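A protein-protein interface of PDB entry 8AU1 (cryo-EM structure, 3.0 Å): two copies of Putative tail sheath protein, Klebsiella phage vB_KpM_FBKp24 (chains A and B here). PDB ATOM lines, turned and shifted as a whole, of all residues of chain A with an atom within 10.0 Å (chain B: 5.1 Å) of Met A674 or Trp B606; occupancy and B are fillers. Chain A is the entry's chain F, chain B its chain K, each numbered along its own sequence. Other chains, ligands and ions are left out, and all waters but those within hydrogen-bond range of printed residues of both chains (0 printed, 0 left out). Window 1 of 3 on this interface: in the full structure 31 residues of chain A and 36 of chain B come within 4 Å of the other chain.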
ATOM      1  N   ARG A 533     -33.810   9.016  16.405  1.00  0.00           N
ATOM      2  CA  ARG A 533     -32.553   8.535  16.961  1.00  0.00           C
ATOM      3  C   ARG A 533     -31.342   8.998  16.165  1.00  0.00           C
ATOM      4  O   ARG A 533     -30.218   8.631  16.519  1.00  0.00           O
ATOM      5  CB  ARG A 533     -32.564   7.009  17.028  1.00  0.00           C
ATOM      6  CG  ARG A 533     -32.417   6.349  15.679  1.00  0.00           C
ATOM      7  CD  ARG A 533     -32.985   4.950  15.677  1.00  0.00           C
ATOM      8  NE  ARG A 533     -32.244   4.061  16.561  1.00  0.00           N
ATOM      9  CZ  ARG A 533     -31.362   3.154  16.162  1.00  0.00           C
ATOM     10  NH1 ARG A 533     -31.065   2.987  14.886  1.00  0.00           N
ATOM     11  NH2 ARG A 533     -30.764   2.393  17.070  1.00  0.00           N
ATOM     12  N   TRP A 548     -11.682   1.997  19.770  1.00  0.00           N
ATOM     13  CA  TRP A 548     -12.574   1.100  20.491  1.00  0.00           C
ATOM     14  C   TRP A 548     -12.385   1.255  21.991  1.00  0.00           C
ATOM     15  O   TRP A 548     -13.350   1.225  22.760  1.00  0.00           O
ATOM     16  CB  TRP A 548     -12.322  -0.343  20.057  1.00  0.00           C
ATOM     17  CG  TRP A 548     -13.054  -1.350  20.871  1.00  0.00           C
ATOM     18  CD1 TRP A 548     -12.522  -2.422  21.514  1.00  0.00           C
ATOM     19  CD2 TRP A 548     -14.461  -1.385  21.130  1.00  0.00           C
ATOM     20  NE1 TRP A 548     -13.506  -3.128  22.157  1.00  0.00           N
ATOM     21  CE2 TRP A 548     -14.706  -2.507  21.938  1.00  0.00           C
ATOM     22  CE3 TRP A 548     -15.533  -0.573  20.760  1.00  0.00           C
ATOM     23  CZ2 TRP A 548     -15.979  -2.839  22.380  1.00  0.00           C
ATOM     24  CZ3 TRP A 548     -16.791  -0.903  21.199  1.00  0.00           C
ATOM     25  CH2 TRP A 548     -17.007  -2.026  22.001  1.00  0.00           C
ATOM     26  N   ARG A 551     -14.122   4.470  23.155  1.00  0.00           N
ATOM     27  CA  ARG A 551     -15.565   4.271  23.221  1.00  0.00           C
ATOM     28  C   ARG A 551     -15.945   3.411  24.419  1.00  0.00           C
ATOM     29  O   ARG A 551     -16.944   3.676  25.095  1.00  0.00           O
ATOM     30  CB  ARG A 551     -16.061   3.646  21.923  1.00  0.00           C
ATOM     31  CG  ARG A 551     -16.537   4.672  20.920  1.00  0.00           C
ATOM     32  CD  ARG A 551     -17.139   4.027  19.700  1.00  0.00           C
ATOM     33  NE  ARG A 551     -16.109   3.469  18.833  1.00  0.00           N
ATOM     34  CZ  ARG A 551     -16.186   2.300  18.213  1.00  0.00           C
ATOM     35  NH1 ARG A 551     -17.245   1.517  18.335  1.00  0.00           N
ATOM     36  NH2 ARG A 551     -15.173   1.906  17.448  1.00  0.00           N
ATOM     37  N   TRP A 555     -18.424   4.620  27.439  1.00  0.00           N
ATOM     38  CA  TRP A 555     -19.613   3.864  27.807  1.00  0.00           C
ATOM     39  C   TRP A 555     -19.574   3.486  29.277  1.00  0.00           C
ATOM     40  O   TRP A 555     -20.569   3.629  29.992  1.00  0.00           O
ATOM     41  CB  TRP A 555     -19.735   2.615  26.942  1.00  0.00           C
ATOM     42  CG  TRP A 555     -20.948   1.802  27.246  1.00  0.00           C
ATOM     43  CD1 TRP A 555     -21.000   0.664  27.988  1.00  0.00           C
ATOM     44  CD2 TRP A 555     -22.288   2.058  26.811  1.00  0.00           C
ATOM     45  NE1 TRP A 555     -22.285   0.193  28.044  1.00  0.00           N
ATOM     46  CE2 TRP A 555     -23.097   1.034  27.331  1.00  0.00           C
ATOM     47  CE3 TRP A 555     -22.881   3.055  26.036  1.00  0.00           C
ATOM     48  CZ2 TRP A 555     -24.464   0.975  27.098  1.00  0.00           C
ATOM     49  CZ3 TRP A 555     -24.237   2.993  25.807  1.00  0.00           C
ATOM     50  CH2 TRP A 555     -25.014   1.962  26.336  1.00  0.00           C
ATOM     51  N   TYR A 561     -22.841   9.509  23.409  1.00  0.00           N
ATOM     52  CA  TYR A 561     -22.075   9.927  22.247  1.00  0.00           C
ATOM     53  C   TYR A 561     -22.736   9.374  20.992  1.00  0.00           C
ATOM     54  O   TYR A 561     -23.561   8.462  21.054  1.00  0.00           O
ATOM     55  CB  TYR A 561     -20.620   9.458  22.344  1.00  0.00           C
ATOM     56  CG  TYR A 561     -20.479   7.973  22.566  1.00  0.00           C
ATOM     57  CD1 TYR A 561     -20.631   7.080  21.523  1.00  0.00           C
ATOM     58  CD2 TYR A 561     -20.192   7.465  23.818  1.00  0.00           C
ATOM     59  CE1 TYR A 561     -20.506   5.730  21.719  1.00  0.00           C
ATOM     60  CE2 TYR A 561     -20.065   6.116  24.025  1.00  0.00           C
ATOM     61  CZ  TYR A 561     -20.223   5.253  22.970  1.00  0.00           C
ATOM     62  OH  TYR A 561     -20.098   3.900  23.164  1.00  0.00           O
ATOM     63  N   VAL A 562     -22.373   9.949  19.849  1.00  0.00           N
ATOM     64  CA  VAL A 562     -22.951   9.568  18.573  1.00  0.00           C
ATOM     65  C   VAL A 562     -21.933   8.764  17.780  1.00  0.00           C
ATOM     66  O   VAL A 562     -20.724   8.841  17.999  1.00  0.00           O
ATOM     67  CB  VAL A 562     -23.419  10.792  17.759  1.00  0.00           C
ATOM     68  CG1 VAL A 562     -24.525  11.516  18.481  1.00  0.00           C
ATOM     69  CG2 VAL A 562     -22.257  11.724  17.480  1.00  0.00           C
ATOM     70  N   GLU A 563     -22.440   7.982  16.834  1.00  0.00           N
ATOM     71  CA  GLU A 563     -21.631   7.239  15.886  1.00  0.00           C
ATOM     72  C   GLU A 563     -22.117   7.559  14.483  1.00  0.00           C
ATOM     73  O   GLU A 563     -23.135   8.224  14.298  1.00  0.00           O
ATOM     74  CB  GLU A 563     -21.716   5.733  16.128  1.00  0.00           C
ATOM     75  CG  GLU A 563     -21.017   5.269  17.376  1.00  0.00           C
ATOM     76  CD  GLU A 563     -20.987   3.763  17.482  1.00  0.00           C
ATOM     77  OE1 GLU A 563     -21.347   3.095  16.494  1.00  0.00           O
ATOM     78  OE2 GLU A 563     -20.607   3.245  18.552  1.00  0.00           O
ATOM     79  N   ASP A 564     -21.374   7.088  13.491  1.00  0.00           N
ATOM     80  CA  ASP A 564     -21.779   7.287  12.109  1.00  0.00           C
ATOM     81  C   ASP A 564     -22.845   6.277  11.718  1.00  0.00           C
ATOM     82  O   ASP A 564     -22.628   5.066  11.796  1.00  0.00           O
ATOM     83  CB  ASP A 564     -20.578   7.163  11.182  1.00  0.00           C
ATOM     84  CG  ASP A 564     -19.660   8.355  11.267  1.00  0.00           C
ATOM     85  OD1 ASP A 564     -19.905   9.347  10.549  1.00  0.00           O
ATOM     86  OD2 ASP A 564     -18.705   8.311  12.065  1.00  0.00           O
ATOM     87  N   TYR A 565     -24.007   6.781  11.310  1.00  0.00           N
ATOM     88  CA  TYR A 565     -25.017   5.927  10.702  1.00  0.00           C
ATOM     89  C   TYR A 565     -24.567   5.490   9.315  1.00  0.00           C
ATOM     90  O   TYR A 565     -24.620   4.307   8.970  1.00  0.00           O
ATOM     91  CB  TYR A 565     -26.350   6.675  10.637  1.00  0.00           C
ATOM     92  CG  TYR A 565     -27.506   5.853  10.137  1.00  0.00           C
ATOM     93  CD1 TYR A 565     -28.013   4.816  10.894  1.00  0.00           C
ATOM     94  CD2 TYR A 565     -28.111   6.136   8.928  1.00  0.00           C
ATOM     95  CE1 TYR A 565     -29.073   4.066  10.451  1.00  0.00           C
ATOM     96  CE2 TYR A 565     -29.175   5.390   8.475  1.00  0.00           C
ATOM     97  CZ  TYR A 565     -29.650   4.355   9.241  1.00  0.00           C
ATOM     98  OH  TYR A 565     -30.710   3.607   8.799  1.00  0.00           O
ATOM     99  N   ASP A 566     -24.111   6.444   8.512  1.00  0.00           N
ATOM    100  CA  ASP A 566     -23.575   6.178   7.189  1.00  0.00           C
ATOM    101  C   ASP A 566     -22.659   7.338   6.821  1.00  0.00           C
ATOM    102  O   ASP A 566     -22.259   8.133   7.676  1.00  0.00           O
ATOM    103  CB  ASP A 566     -24.708   5.965   6.179  1.00  0.00           C
ATOM    104  CG  ASP A 566     -25.615   7.159   6.067  1.00  0.00           C
ATOM    105  OD1 ASP A 566     -25.289   8.206   6.656  1.00  0.00           O
ATOM    106  OD2 ASP A 566     -26.657   7.056   5.391  1.00  0.00           O
ATOM    107  N   PHE A 571     -25.964   8.712  14.548  1.00  0.00           N
ATOM    108  CA  PHE A 571     -27.086   8.247  15.350  1.00  0.00           C
ATOM    109  C   PHE A 571     -26.604   7.936  16.760  1.00  0.00           C
ATOM    110  O   PHE A 571     -25.404   7.928  17.039  1.00  0.00           O
ATOM    111  CB  PHE A 571     -27.756   7.011  14.729  1.00  0.00           C
ATOM    112  CG  PHE A 571     -26.960   5.744  14.852  1.00  0.00           C
ATOM    113  CD1 PHE A 571     -26.005   5.407  13.924  1.00  0.00           C
ATOM    114  CD2 PHE A 571     -27.223   4.854  15.871  1.00  0.00           C
ATOM    115  CE1 PHE A 571     -25.301   4.234  14.039  1.00  0.00           C
ATOM    116  CE2 PHE A 571     -26.521   3.681  15.983  1.00  0.00           C
ATOM    117  CZ  PHE A 571     -25.562   3.372  15.066  1.00  0.00           C
ATOM    118  N   TYR A 572     -27.562   7.685  17.657  1.00  0.00           N
ATOM    119  CA  TYR A 572     -27.260   7.387  19.049  1.00  0.00           C
ATOM    120  C   TYR A 572     -27.375   5.892  19.287  1.00  0.00           C
ATOM    121  O   TYR A 572     -28.498   5.368  19.319  1.00  0.00           O
ATOM    122  CB  TYR A 572     -28.209   8.142  19.976  1.00  0.00           C
ATOM    123  CG  TYR A 572     -28.004   9.632  19.964  1.00  0.00           C
ATOM    124  CD1 TYR A 572     -28.579  10.417  18.984  1.00  0.00           C
ATOM    125  CD2 TYR A 572     -27.233  10.252  20.931  1.00  0.00           C
ATOM    126  CE1 TYR A 572     -28.392  11.778  18.965  1.00  0.00           C
ATOM    127  CE2 TYR A 572     -27.039  11.615  20.918  1.00  0.00           C
ATOM    128  CZ  TYR A 572     -27.620  12.372  19.930  1.00  0.00           C
ATOM    129  OH  TYR A 572     -27.435  13.730  19.909  1.00  0.00           O
ATOM    130  N   PRO A 573     -26.272   5.163  19.475  1.00  0.00           N
ATOM    131  CA  PRO A 573     -26.392   3.730  19.770  1.00  0.00           C
ATOM    132  C   PRO A 573     -27.186   3.437  21.027  1.00  0.00           C
ATOM    133  O   PRO A 573     -27.875   2.413  21.077  1.00  0.00           O
ATOM    134  CB  PRO A 573     -24.933   3.279  19.914  1.00  0.00           C
ATOM    135  CG  PRO A 573     -24.151   4.292  19.194  1.00  0.00           C
ATOM    136  CD  PRO A 573     -24.865   5.579  19.404  1.00  0.00           C
ATOM    137  N   GLY A 574     -27.116   4.295  22.037  1.00  0.00           N
ATOM    138  CA  GLY A 574     -27.846   4.089  23.269  1.00  0.00           C
ATOM    139  C   GLY A 574     -27.820   5.334  24.125  1.00  0.00           C
ATOM    140  O   GLY A 574     -26.756   5.917  24.340  1.00  0.00           O
ATOM    141  N   ARG A 671     -31.157  -4.065  24.824  1.00  0.00           N
ATOM    142  CA  ARG A 671     -30.026  -4.868  24.375  1.00  0.00           C
ATOM    143  C   ARG A 671     -29.229  -4.092  23.336  1.00  0.00           C
ATOM    144  O   ARG A 671     -29.790  -3.283  22.595  1.00  0.00           O
ATOM    145  CB  ARG A 671     -30.506  -6.191  23.783  1.00  0.00           C
ATOM    146  CG  ARG A 671     -31.489  -6.946  24.653  1.00  0.00           C
ATOM    147  CD  ARG A 671     -31.998  -8.187  23.957  1.00  0.00           C
ATOM    148  NE  ARG A 671     -31.416  -9.407  24.504  1.00  0.00           N
ATOM    149  CZ  ARG A 671     -31.957 -10.137  25.469  1.00  0.00           C
ATOM    150  NH1 ARG A 671     -33.087  -9.782  26.055  1.00  0.00           N
ATOM    151  NH2 ARG A 671     -31.347 -11.249  25.860  1.00  0.00           N
ATOM    152  N   THR A 672     -27.916  -4.339  23.278  1.00  0.00           N
ATOM    153  CA  THR A 672     -27.036  -3.520  22.454  1.00  0.00           C
ATOM    154  C   THR A 672     -25.925  -4.261  21.716  1.00  0.00           C
ATOM    155  O   THR A 672     -25.098  -3.594  21.090  1.00  0.00           O
ATOM    156  CB  THR A 672     -26.381  -2.421  23.308  1.00  0.00           C
ATOM    157  OG1 THR A 672     -25.740  -3.007  24.447  1.00  0.00           O
ATOM    158  CG2 THR A 672     -27.412  -1.419  23.786  1.00  0.00           C
ATOM    159  N   VAL A 673     -25.863  -5.590  21.757  1.00  0.00           N
ATOM    160  CA  VAL A 673     -24.734  -6.330  21.198  1.00  0.00           C
ATOM    161  C   VAL A 673     -25.249  -7.446  20.300  1.00  0.00           C
ATOM    162  O   VAL A 673     -26.265  -8.078  20.602  1.00  0.00           O
ATOM    163  CB  VAL A 673     -23.835  -6.901  22.312  1.00  0.00           C
ATOM    164  CG1 VAL A 673     -22.677  -7.673  21.721  1.00  0.00           C
ATOM    165  CG2 VAL A 673     -23.327  -5.786  23.199  1.00  0.00           C
ATOM    166  N   MET A 674     -24.537  -7.693  19.200  1.00  0.00           N
ATOM    167  CA  MET A 674     -24.881  -8.743  18.251  1.00  0.00           C
ATOM    168  C   MET A 674     -23.681  -9.646  18.004  1.00  0.00           C
ATOM    169  O   MET A 674     -22.536  -9.190  18.019  1.00  0.00           O
ATOM    170  CB  MET A 674     -25.336  -8.176  16.906  1.00  0.00           C
ATOM    171  CG  MET A 674     -25.814  -9.250  15.931  1.00  0.00           C
ATOM    172  SD  MET A 674     -26.362  -8.641  14.331  1.00  0.00           S
ATOM    173  CE  MET A 674     -27.897  -7.863  14.769  1.00  0.00           C
ATOM    174  N   ASP A 675     -23.956 -10.921  17.761  1.00  0.00           N
ATOM    175  CA  ASP A 675     -22.970 -11.887  17.308  1.00  0.00           C
ATOM    176  C   ASP A 675     -23.357 -12.416  15.936  1.00  0.00           C
ATOM    177  O   ASP A 675     -24.534 -12.610  15.633  1.00  0.00           O
ATOM    178  CB  ASP A 675     -22.858 -13.051  18.285  1.00  0.00           C
ATOM    179  CG  ASP A 675     -22.306 -12.633  19.611  1.00  0.00           C
ATOM    180  OD1 ASP A 675     -22.306 -11.417  19.883  1.00  0.00           O
ATOM    181  OD2 ASP A 675     -21.877 -13.514  20.381  1.00  0.00           O
ATOM    182  N   MET A 676     -22.349 -12.656  15.105  1.00  0.00           N
ATOM    183  CA  MET A 676     -22.599 -13.207  13.785  1.00  0.00           C
ATOM    184  C   MET A 676     -21.650 -14.359  13.510  1.00  0.00           C
ATOM    185  O   MET A 676     -20.494 -14.341  13.935  1.00  0.00           O
ATOM    186  CB  MET A 676     -22.442 -12.156  12.688  1.00  0.00           C
ATOM    187  CG  MET A 676     -22.778 -12.710  11.324  1.00  0.00           C
ATOM    188  SD  MET A 676     -22.692 -11.501  10.019  1.00  0.00           S
ATOM    189  CE  MET A 676     -23.038 -12.551   8.622  1.00  0.00           C
ATOM    190  N   SER A 677     -22.151 -15.349  12.778  1.00  0.00           N
ATOM    191  CA  SER A 677     -21.363 -16.491  12.361  1.00  0.00           C
ATOM    192  C   SER A 677     -21.891 -16.969  11.021  1.00  0.00           C
ATOM    193  O   SER A 677     -22.877 -16.446  10.500  1.00  0.00           O
ATOM    194  CB  SER A 677     -21.419 -17.619  13.387  1.00  0.00           C
ATOM    195  OG  SER A 677     -20.917 -17.185  14.633  1.00  0.00           O
ATOM    196  N   ALA B 602     -25.403  -7.845   7.626  1.00  0.00           N
ATOM    197  CA  ALA B 602     -25.590  -8.075   9.060  1.00  0.00           C
ATOM    198  C   ALA B 602     -25.288  -6.821   9.876  1.00  0.00           C
ATOM    199  O   ALA B 602     -26.008  -6.502  10.835  1.00  0.00           O
ATOM    200  CB  ALA B 602     -24.709  -9.223   9.526  1.00  0.00           C
ATOM    201  N   PHE B 603     -24.216  -6.110   9.530  1.00  0.00           N
ATOM    202  CA  PHE B 603     -23.905  -4.865  10.218  1.00  0.00           C
ATOM    203  C   PHE B 603     -25.060  -3.890  10.101  1.00  0.00           C
ATOM    204  O   PHE B 603     -25.395  -3.189  11.058  1.00  0.00           O
ATOM    205  CB  PHE B 603     -22.635  -4.241   9.642  1.00  0.00           C
ATOM    206  CG  PHE B 603     -22.502  -2.772   9.926  1.00  0.00           C
ATOM    207  CD1 PHE B 603     -21.993  -2.328  11.128  1.00  0.00           C
ATOM    208  CD2 PHE B 603     -22.895  -1.836   8.992  1.00  0.00           C
ATOM    209  CE1 PHE B 603     -21.879  -0.982  11.387  1.00  0.00           C
ATOM    210  CE2 PHE B 603     -22.782  -0.494   9.251  1.00  0.00           C
ATOM    211  CZ  PHE B 603     -22.271  -0.067  10.445  1.00  0.00           C
ATOM    212  N   GLU B 604     -25.666  -3.811   8.916  1.00  0.00           N
ATOM    213  CA  GLU B 604     -26.795  -2.899   8.745  1.00  0.00           C
ATOM    214  C   GLU B 604     -27.955  -3.282   9.655  1.00  0.00           C
ATOM    215  O   GLU B 604     -28.603  -2.412  10.252  1.00  0.00           O
ATOM    216  CB  GLU B 604     -27.245  -2.888   7.290  1.00  0.00           C
ATOM    217  CG  GLU B 604     -26.297  -2.159   6.375  1.00  0.00           C
ATOM    218  CD  GLU B 604     -26.772  -2.169   4.950  1.00  0.00           C
ATOM    219  OE1 GLU B 604     -27.861  -2.716   4.699  1.00  0.00           O
ATOM    220  OE2 GLU B 604     -26.061  -1.634   4.078  1.00  0.00           O
ATOM    221  N   ALA B 605     -28.232  -4.579   9.774  1.00  0.00           N
ATOM    222  CA  ALA B 605     -29.295  -5.019  10.676  1.00  0.00           C
ATOM    223  C   ALA B 605     -29.023  -4.567  12.106  1.00  0.00           C
ATOM    224  O   ALA B 605     -29.908  -4.025  12.784  1.00  0.00           O
ATOM    225  CB  ALA B 605     -29.437  -6.537  10.620  1.00  0.00           C
ATOM    226  N   TRP B 606     -27.798  -4.789  12.587  1.00  0.00           N
ATOM    227  CA  TRP B 606     -27.459  -4.338  13.936  1.00  0.00           C
ATOM    228  C   TRP B 606     -27.646  -2.835  14.069  1.00  0.00           C
ATOM    229  O   TRP B 606     -28.266  -2.347  15.023  1.00  0.00           O
ATOM    230  CB  TRP B 606     -26.019  -4.697  14.287  1.00  0.00           C
ATOM    231  CG  TRP B 606     -25.575  -4.016  15.544  1.00  0.00           C
ATOM    232  CD1 TRP B 606     -25.749  -4.463  16.812  1.00  0.00           C
ATOM    233  CD2 TRP B 606     -24.913  -2.748  15.655  1.00  0.00           C
ATOM    234  NE1 TRP B 606     -25.230  -3.567  17.705  1.00  0.00           N
ATOM    235  CE2 TRP B 606     -24.713  -2.503  17.019  1.00  0.00           C
ATOM    236  CE3 TRP B 606     -24.467  -1.801  14.732  1.00  0.00           C
ATOM    237  CZ2 TRP B 606     -24.087  -1.356  17.485  1.00  0.00           C
ATOM    238  CZ3 TRP B 606     -23.845  -0.659  15.201  1.00  0.00           C
ATOM    239  CH2 TRP B 606     -23.664  -0.448  16.560  1.00  0.00           C
ATOM    240  N   ARG B 607     -27.094  -2.086  13.119  1.00  0.00           N
ATOM    241  CA  ARG B 607     -27.131  -0.634  13.185  1.00  0.00           C
ATOM    242  C   ARG B 607     -28.559  -0.138  13.275  1.00  0.00           C
ATOM    243  O   ARG B 607     -28.832   0.881  13.916  1.00  0.00           O
ATOM    244  CB  ARG B 607     -26.427  -0.063  11.956  1.00  0.00           C
ATOM    245  CG  ARG B 607     -26.499   1.435  11.781  1.00  0.00           C
ATOM    246  CD  ARG B 607     -26.136   1.795  10.357  1.00  0.00           C
ATOM    247  NE  ARG B 607     -27.154   1.344   9.417  1.00  0.00           N
ATOM    248  CZ  ARG B 607     -27.225   1.718   8.148  1.00  0.00           C
ATOM    249  NH1 ARG B 607     -26.301   2.485   7.600  1.00  0.00           N
ATOM    250  NH2 ARG B 607     -28.247   1.303   7.408  1.00  0.00           N
ATOM    251  N   ASP B 608     -29.486  -0.841  12.630  1.00  0.00           N
ATOM    252  CA  ASP B 608     -30.883  -0.435  12.711  1.00  0.00           C
ATOM    253  C   ASP B 608     -31.512  -0.793  14.051  1.00  0.00           C
ATOM    254  O   ASP B 608     -32.275   0.002  14.605  1.00  0.00           O
ATOM    255  CB  ASP B 608     -31.679  -1.064  11.574  1.00  0.00           C
ATOM    256  CG  ASP B 608     -31.631  -0.237  10.317  1.00  0.00           C
ATOM    257  OD1 ASP B 608     -32.098   0.919  10.352  1.00  0.00           O
ATOM    258  OD2 ASP B 608     -31.122  -0.737   9.295  1.00  0.00           O
ATOM    259  N   LEU B 609     -31.217  -1.974  14.591  1.00  0.00           N
ATOM    260  CA  LEU B 609     -31.975  -2.459  15.739  1.00  0.00           C
ATOM    261  C   LEU B 609     -31.391  -2.075  17.095  1.00  0.00           C
ATOM    262  O   LEU B 609     -32.069  -2.267  18.108  1.00  0.00           O
ATOM    263  CB  LEU B 609     -32.103  -3.982  15.675  1.00  0.00           C
ATOM    264  CG  LEU B 609     -33.113  -4.498  14.655  1.00  0.00           C
ATOM    265  CD1 LEU B 609     -32.808  -5.937  14.316  1.00  0.00           C
ATOM    266  CD2 LEU B 609     -34.525  -4.361  15.182  1.00  0.00           C
ATOM    267  N   THR B 610     -30.174  -1.547  17.156  1.00  0.00           N
ATOM    268  CA  THR B 610     -29.523  -1.351  18.448  1.00  0.00           C
ATOM    269  C   THR B 610     -30.256  -0.340  19.330  1.00  0.00           C
ATOM    270  O   THR B 610     -30.804   0.658  18.856  1.00  0.00           O
ATOM    271  CB  THR B 610     -28.082  -0.886  18.260  1.00  0.00           C
ATOM    272  OG1 THR B 610     -27.488  -0.661  19.541  1.00  0.00           O
ATOM    273  CG2 THR B 610     -28.024   0.395  17.462  1.00  0.00           C
ATOM    274  N   SER B 624     -34.471  -8.835  12.783  1.00  0.00           N
ATOM    275  CA  SER B 624     -33.121  -9.036  12.261  1.00  0.00           C
ATOM    276  C   SER B 624     -33.133  -9.878  10.986  1.00  0.00           C
ATOM    277  O   SER B 624     -32.564  -9.483   9.956  1.00  0.00           O
ATOM    278  CB  SER B 624     -32.251  -9.685  13.328  1.00  0.00           C
ATOM    279  OG  SER B 624     -32.069  -8.799  14.412  1.00  0.00           O
ATOM    280  N   TRP B 659     -27.898 -10.616  21.412  1.00  0.00           N
ATOM    281  CA  TRP B 659     -28.610 -11.633  20.651  1.00  0.00           C
ATOM    282  C   TRP B 659     -27.728 -12.067  19.489  1.00  0.00           C
ATOM    283  O   TRP B 659     -26.787 -11.370  19.113  1.00  0.00           O
ATOM    284  CB  TRP B 659     -29.971 -11.128  20.159  1.00  0.00           C
ATOM    285  CG  TRP B 659     -29.944 -10.168  19.006  1.00  0.00           C
ATOM    286  CD1 TRP B 659     -30.247 -10.450  17.712  1.00  0.00           C
ATOM    287  CD2 TRP B 659     -29.626  -8.771  19.045  1.00  0.00           C
ATOM    288  NE1 TRP B 659     -30.131  -9.326  16.941  1.00  0.00           N
ATOM    289  CE2 TRP B 659     -29.748  -8.282  17.738  1.00  0.00           C
ATOM    290  CE3 TRP B 659     -29.244  -7.891  20.059  1.00  0.00           C
ATOM    291  CZ2 TRP B 659     -29.504  -6.953  17.416  1.00  0.00           C
ATOM    292  CZ3 TRP B 659     -29.003  -6.577  19.735  1.00  0.00           C
ATOM    293  CH2 TRP B 659     -29.134  -6.119  18.428  1.00  0.00           C
ATOM    294  N   MET B 661     -26.996 -13.910  15.549  1.00  0.00           N
ATOM    295  CA  MET B 661     -27.398 -14.179  14.178  1.00  0.00           C
ATOM    296  C   MET B 661     -26.450 -15.206  13.577  1.00  0.00           C
ATOM    297  O   MET B 661     -25.281 -15.286  13.955  1.00  0.00           O
ATOM    298  CB  MET B 661     -27.376 -12.922  13.309  1.00  0.00           C
ATOM    299  CG  MET B 661     -27.907 -13.149  11.900  1.00  0.00           C
ATOM    300  SD  MET B 661     -27.891 -11.677  10.873  1.00  0.00           S
ATOM    301  CE  MET B 661     -29.209 -10.729  11.602  1.00  0.00           C
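OH of Tyr A565 is in hydrogen-bond range of OD1 of Asp B608 (3.4 Å). NH2 of Arg A533 is in hydrogen-bond range of O of Thr B610 (2.5 Å). O of Asp A675 lies within hydrogen-bond range of N of Met B661, 2.8 Å away. The backbone NH (N) of Asp A675 sits at hydrogen-bond distance from the backbone carbonyl oxygen (O) of Trp B659, at 3.2 Å. The backbone carbonyl oxygen (O) of Tyr A565 sits at hydrogen-bond distance from the guanidinium group (NH1) of Arg B607 (2.8 Å). The backbone carbonyl oxygen of Pro A573 is in hydrogen-bond range of the side-chain hydroxyl of Thr B610 (3.5 Å). The guanidinium group of Arg A533 is in hydrogen-bond range of the backbone carbonyl oxygen of Asp B608 (3.2 Å). O of Met B661 is in hydrogen-bond range of N of Ser A677 (3.3 Å). NH1 of Arg A533 lies within hydrogen-bond range of O of Arg B607 (3.2 Å). O of Val A673 sits close to N of Trp B659 (3.1 Å). The indole nitrogen of Trp B606 lies within hydrogen-bond range of the backbone carbonyl oxygen of Thr A672 (3.4 Å).
Arg B607 touches Phe A571. Thr B610 touches Phe A571. Met A674 touches Trp B606. Met A674 touches Trp B659 (CE to CZ2, 3.2 Å). Met A676 touches Ala B602. Met B661 touches Met A676.
Of the 12 printed residues of chain B, 7 touch a printed residue of chain A. Hydrophobic or aromatic side chains of chain B that line the printed part of chain A: Ala B602, Trp B606, Trp B659 and Met B661. Hydrophobic or aromatic side chains of chain A within 4 Å of the printed part of chain B: Tyr A565, Phe A571, Met A674 and Met A676.
The backbone NH (N) of Phe A571 sits at hydrogen-bond distance from the backbone carbonyl oxygen (O) of Glu A563. The side-chain hydroxyl (OG) of Ser B624 sits at hydrogen-bond distance from the indole nitrogen (NE1) of Trp B659 (3.2 Å). The backbone NH of Tyr A572 sits at hydrogen-bond distance from the backbone carbonyl oxygen of Arg A533 (3.0 Å). NH2 of Arg B607 is in salt-bridge range of OD2 of Asp B608, 3.998 Å away.
No position is printed for both chains.
Of chain B, only Trp B606 and Trp B659 come within 4 Å of Met A674. Of chain A, only Thr A672 (3.4 Å) and Met A674 (3.6 Å) come within 4 Å of Trp B606. Thr B610 touches just these residues of chain A: Arg A533, Phe A571 and Pro A573. Trp B659 touches three residues of chain A. Printed residues of chain B within 4 Å of Thr A672: Trp B606. Of the printed residues of chain B, Pro A573 touches Thr B610 (3.5 Å). Of the printed residues of chain B, Ser A677 touches Met B661. The nearest residue of chain B that does not touch Met A674 is Ala B602 (4.1 Å). The nearest residue of chain A that does not touch Trp B606 is Glu A563 (4.2 Å).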
